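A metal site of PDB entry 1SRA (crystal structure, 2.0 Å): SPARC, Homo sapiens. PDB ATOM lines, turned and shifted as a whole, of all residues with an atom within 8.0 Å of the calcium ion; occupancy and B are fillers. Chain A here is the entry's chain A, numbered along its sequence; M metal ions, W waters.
Five residues have an atom within 4 Å of the calcium ion: Asp 87, Pro 90, Asp 92, Tyr 94 and Glu 99. The nearest printed residue that does not touch the calcium ion is Gln 88 (4.4 Å).
The backbone NH (N) of His 89 lies close to the side-chain carboxylate (OE2) of Glu 99 (2.7 Å). The backbone NH (N) of Glu 99 sits at hydrogen-bond distance from the side-chain hydroxyl (OG) of Ser 96 (3.3 Å). OE2 of Glu 99 lies close to N of Gln 88 (2.8 Å). The side-chain carboxylate (OD2) of Asp 87 is in hydrogen-bond range of the backbone NH (N) of Gly 93, at 2.8 Å.
The calcium ion is bound by the side-chain carboxylate (OD1) of Asp 87 (2.1 Å), water W1 (2.2 Å), the backbone carbonyl oxygen (O) of Pro 90 (2.4 Å), the side-chain carboxylate (OD1) of Asp 92 (2.4 Å), the backbone carbonyl oxygen (O) of Tyr 94 (2.4 Å), the side-chain carboxylate (OE2) of Glu 99 (2.6 Å) and the side-chain carboxylate (OE1) of Glu 99 (2.6 Å). The calcium ion has seven donor atoms within binding distance.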
ATOM      1  N   PHE A  83      -2.738  21.608   2.907  1.00  0.00           N
ATOM      2  CA  PHE A  83      -3.685  22.658   3.320  1.00  0.00           C
ATOM      3  C   PHE A  83      -5.072  22.334   2.767  1.00  0.00           C
ATOM      4  O   PHE A  83      -6.074  22.433   3.476  1.00  0.00           O
ATOM      5  CB  PHE A  83      -3.233  24.051   2.795  1.00  0.00           C
ATOM      6  CG  PHE A  83      -4.091  25.195   3.290  1.00  0.00           C
ATOM      7  CD1 PHE A  83      -5.265  25.551   2.624  1.00  0.00           C
ATOM      8  CD2 PHE A  83      -3.739  25.912   4.427  1.00  0.00           C
ATOM      9  CE1 PHE A  83      -6.066  26.606   3.072  1.00  0.00           C
ATOM     10  CE2 PHE A  83      -4.519  26.967   4.903  1.00  0.00           C
ATOM     11  CZ  PHE A  83      -5.687  27.321   4.218  1.00  0.00           C
ATOM     12  N   LEU A  86      -7.005  19.731   4.752  1.00  0.00           N
ATOM     13  CA  LEU A  86      -7.538  20.123   6.049  1.00  0.00           C
ATOM     14  C   LEU A  86      -8.643  21.175   5.982  1.00  0.00           C
ATOM     15  O   LEU A  86      -9.489  21.244   6.870  1.00  0.00           O
ATOM     16  CB  LEU A  86      -6.379  20.634   6.933  1.00  0.00           C
ATOM     17  CG  LEU A  86      -5.236  19.659   7.256  1.00  0.00           C
ATOM     18  CD1 LEU A  86      -4.091  20.354   7.990  1.00  0.00           C
ATOM     19  CD2 LEU A  86      -5.781  18.514   8.105  1.00  0.00           C
ATOM     20  N   ASP A  87      -8.639  22.005   4.947  1.00  0.00           N
ATOM     21  CA  ASP A  87      -9.636  23.077   4.848  1.00  0.00           C
ATOM     22  C   ASP A  87     -10.936  22.503   4.359  1.00  0.00           C
ATOM     23  O   ASP A  87     -11.244  22.570   3.182  1.00  0.00           O
ATOM     24  CB  ASP A  87      -9.127  24.148   3.901  1.00  0.00           C
ATOM     25  CG  ASP A  87     -10.001  25.367   3.888  1.00  0.00           C
ATOM     26  OD1 ASP A  87     -10.786  25.597   4.851  1.00  0.00           O
ATOM     27  OD2 ASP A  87      -9.870  26.097   2.892  1.00  0.00           O
ATOM     28  N   GLN A  88     -11.781  22.082   5.289  1.00  0.00           N
ATOM     29  CA  GLN A  88     -13.006  21.418   4.864  1.00  0.00           C
ATOM     30  C   GLN A  88     -14.244  21.780   5.651  1.00  0.00           C
ATOM     31  O   GLN A  88     -15.354  21.521   5.208  1.00  0.00           O
ATOM     32  CB  GLN A  88     -12.825  19.912   5.030  1.00  0.00           C
ATOM     33  CG  GLN A  88     -11.700  19.306   4.234  1.00  0.00           C
ATOM     34  CD  GLN A  88     -12.096  19.073   2.789  1.00  0.00           C
ATOM     35  OE1 GLN A  88     -13.266  18.832   2.494  1.00  0.00           O
ATOM     36  NE2 GLN A  88     -11.123  19.124   1.896  1.00  0.00           N
ATOM     37  N   HIS A  89     -14.055  22.350   6.828  1.00  0.00           N
ATOM     38  CA  HIS A  89     -15.165  22.616   7.696  1.00  0.00           C
ATOM     39  C   HIS A  89     -15.286  23.996   8.321  1.00  0.00           C
ATOM     40  O   HIS A  89     -15.140  24.122   9.510  1.00  0.00           O
ATOM     41  CB  HIS A  89     -15.149  21.582   8.813  1.00  0.00           C
ATOM     42  CG  HIS A  89     -15.011  20.180   8.312  1.00  0.00           C
ATOM     43  ND1 HIS A  89     -13.925  19.389   8.618  1.00  0.00           N
ATOM     44  CD2 HIS A  89     -15.800  19.441   7.504  1.00  0.00           C
ATOM     45  CE1 HIS A  89     -14.043  18.228   8.022  1.00  0.00           C
ATOM     46  NE2 HIS A  89     -15.174  18.220   7.335  1.00  0.00           N
ATOM     47  N   PRO A  90     -15.653  25.018   7.528  1.00  0.00           N
ATOM     48  CA  PRO A  90     -15.944  24.865   6.086  1.00  0.00           C
ATOM     49  C   PRO A  90     -14.718  25.177   5.212  1.00  0.00           C
ATOM     50  O   PRO A  90     -13.700  25.679   5.695  1.00  0.00           O
ATOM     51  CB  PRO A  90     -17.016  25.952   5.857  1.00  0.00           C
ATOM     52  CG  PRO A  90     -16.445  27.127   6.676  1.00  0.00           C
ATOM     53  CD  PRO A  90     -16.030  26.378   8.012  1.00  0.00           C
ATOM     54  N   ILE A  91     -14.825  24.903   3.924  1.00  0.00           N
ATOM     55  CA  ILE A  91     -13.742  25.233   3.035  1.00  0.00           C
ATOM     56  C   ILE A  91     -13.858  26.763   2.835  1.00  0.00           C
ATOM     57  O   ILE A  91     -14.893  27.259   2.386  1.00  0.00           O
ATOM     58  CB  ILE A  91     -13.843  24.449   1.720  1.00  0.00           C
ATOM     59  CG1 ILE A  91     -12.770  24.953   0.757  1.00  0.00           C
ATOM     60  CG2 ILE A  91     -15.227  24.600   1.106  1.00  0.00           C
ATOM     61  CD1 ILE A  91     -12.813  24.337  -0.611  1.00  0.00           C
ATOM     62  N   ASP A  92     -12.844  27.505   3.270  1.00  0.00           N
ATOM     63  CA  ASP A  92     -12.874  28.962   3.198  1.00  0.00           C
ATOM     64  C   ASP A  92     -11.501  29.613   3.070  1.00  0.00           C
ATOM     65  O   ASP A  92     -11.395  30.842   3.171  1.00  0.00           O
ATOM     66  CB  ASP A  92     -13.590  29.504   4.465  1.00  0.00           C
ATOM     67  CG  ASP A  92     -12.880  29.108   5.770  1.00  0.00           C
ATOM     68  OD1 ASP A  92     -11.898  28.349   5.715  1.00  0.00           O
ATOM     69  OD2 ASP A  92     -13.287  29.563   6.858  1.00  0.00           O
ATOM     70  N   GLY A  93     -10.452  28.813   2.861  1.00  0.00           N
ATOM     71  CA  GLY A  93      -9.093  29.347   2.763  1.00  0.00           C
ATOM     72  C   GLY A  93      -8.402  29.599   4.108  1.00  0.00           C
ATOM     73  O   GLY A  93      -7.339  30.209   4.162  1.00  0.00           O
ATOM     74  N   TYR A  94      -9.010  29.151   5.199  1.00  0.00           N
ATOM     75  CA  TYR A  94      -8.433  29.303   6.541  1.00  0.00           C
ATOM     76  C   TYR A  94      -8.534  27.957   7.265  1.00  0.00           C
ATOM     77  O   TYR A  94      -9.358  27.104   6.922  1.00  0.00           O
ATOM     78  CB  TYR A  94      -9.193  30.324   7.406  1.00  0.00           C
ATOM     79  CG  TYR A  94      -9.231  31.704   6.824  1.00  0.00           C
ATOM     80  CD1 TYR A  94     -10.181  32.017   5.843  1.00  0.00           C
ATOM     81  CD2 TYR A  94      -8.244  32.656   7.133  1.00  0.00           C
ATOM     82  CE1 TYR A  94     -10.141  33.246   5.175  1.00  0.00           C
ATOM     83  CE2 TYR A  94      -8.196  33.891   6.468  1.00  0.00           C
ATOM     84  CZ  TYR A  94      -9.150  34.176   5.488  1.00  0.00           C
ATOM     85  OH  TYR A  94      -9.125  35.368   4.789  1.00  0.00           O
ATOM     86  N   LEU A  95      -7.662  27.769   8.251  1.00  0.00           N
ATOM     87  CA  LEU A  95      -7.667  26.545   9.044  1.00  0.00           C
ATOM     88  C   LEU A  95      -7.913  26.917  10.486  1.00  0.00           C
ATOM     89  O   LEU A  95      -7.175  27.698  11.073  1.00  0.00           O
ATOM     90  CB  LEU A  95      -6.330  25.792   8.909  1.00  0.00           C
ATOM     91  CG  LEU A  95      -5.879  25.277   7.546  1.00  0.00           C
ATOM     92  CD1 LEU A  95      -4.665  24.406   7.754  1.00  0.00           C
ATOM     93  CD2 LEU A  95      -6.966  24.438   6.910  1.00  0.00           C
ATOM     94  N   SER A  96      -9.007  26.423  11.031  1.00  0.00           N
ATOM     95  CA  SER A  96      -9.336  26.687  12.416  1.00  0.00           C
ATOM     96  C   SER A  96      -8.579  25.664  13.298  1.00  0.00           C
ATOM     97  O   SER A  96      -7.930  24.740  12.809  1.00  0.00           O
ATOM     98  CB  SER A  96     -10.842  26.539  12.638  1.00  0.00           C
ATOM     99  OG  SER A  96     -11.279  25.190  12.458  1.00  0.00           O
ATOM    100  N   GLU A  99      -9.912  22.240  12.547  1.00  0.00           N
ATOM    101  CA  GLU A  99      -9.482  21.672  11.300  1.00  0.00           C
ATOM    102  C   GLU A  99      -8.027  21.177  11.395  1.00  0.00           C
ATOM    103  O   GLU A  99      -7.585  20.365  10.588  1.00  0.00           O
ATOM    104  CB  GLU A  99      -9.663  22.704  10.164  1.00  0.00           C
ATOM    105  CG  GLU A  99     -11.126  22.849   9.631  1.00  0.00           C
ATOM    106  CD  GLU A  99     -11.232  23.971   8.593  1.00  0.00           C
ATOM    107  OE1 GLU A  99     -10.669  25.053   8.851  1.00  0.00           O
ATOM    108  OE2 GLU A  99     -11.885  23.785   7.547  1.00  0.00           O
ATOM    109  N   TYR A 128      -6.851  31.635  13.276  1.00  0.00           N
ATOM    110  CA  TYR A 128      -7.097  30.815  12.098  1.00  0.00           C
ATOM    111  C   TYR A 128      -5.845  30.906  11.277  1.00  0.00           C
ATOM    112  O   TYR A 128      -5.131  31.899  11.361  1.00  0.00           O
ATOM    113  CB  TYR A 128      -8.285  31.356  11.282  1.00  0.00           C
ATOM    114  CG  TYR A 128      -9.641  30.900  11.794  1.00  0.00           C
ATOM    115  CD1 TYR A 128     -10.093  31.307  13.031  1.00  0.00           C
ATOM    116  CD2 TYR A 128     -10.469  30.089  11.013  1.00  0.00           C
ATOM    117  CE1 TYR A 128     -11.340  30.926  13.484  1.00  0.00           C
ATOM    118  CE2 TYR A 128     -11.697  29.705  11.452  1.00  0.00           C
ATOM    119  CZ  TYR A 128     -12.137  30.131  12.680  1.00  0.00           C
ATOM    120  OH  TYR A 128     -13.402  29.800  13.091  1.00  0.00           O
ATOM    121  N   ILE A 129      -5.554  29.893  10.477  1.00  0.00           N
ATOM    122  CA  ILE A 129      -4.345  29.954   9.667  1.00  0.00           C
ATOM    123  C   ILE A 129      -4.759  30.129   8.204  1.00  0.00           C
ATOM    124  O   ILE A 129      -5.347  29.230   7.623  1.00  0.00           O
ATOM    125  CB  ILE A 129      -3.454  28.651   9.852  1.00  0.00           C
ATOM    126  CG1 ILE A 129      -3.106  28.407  11.334  1.00  0.00           C
ATOM    127  CG2 ILE A 129      -2.172  28.738   9.031  1.00  0.00           C
ATOM    128  CD1 ILE A 129      -2.297  29.477  12.007  1.00  0.00           C
HETATM  129 CA    CA M   1     -11.615  26.189   6.740  1.00  0.00          CA
HETATM  130  O   HOH W   1     -12.461  27.447   8.300  1.00  0.00           O
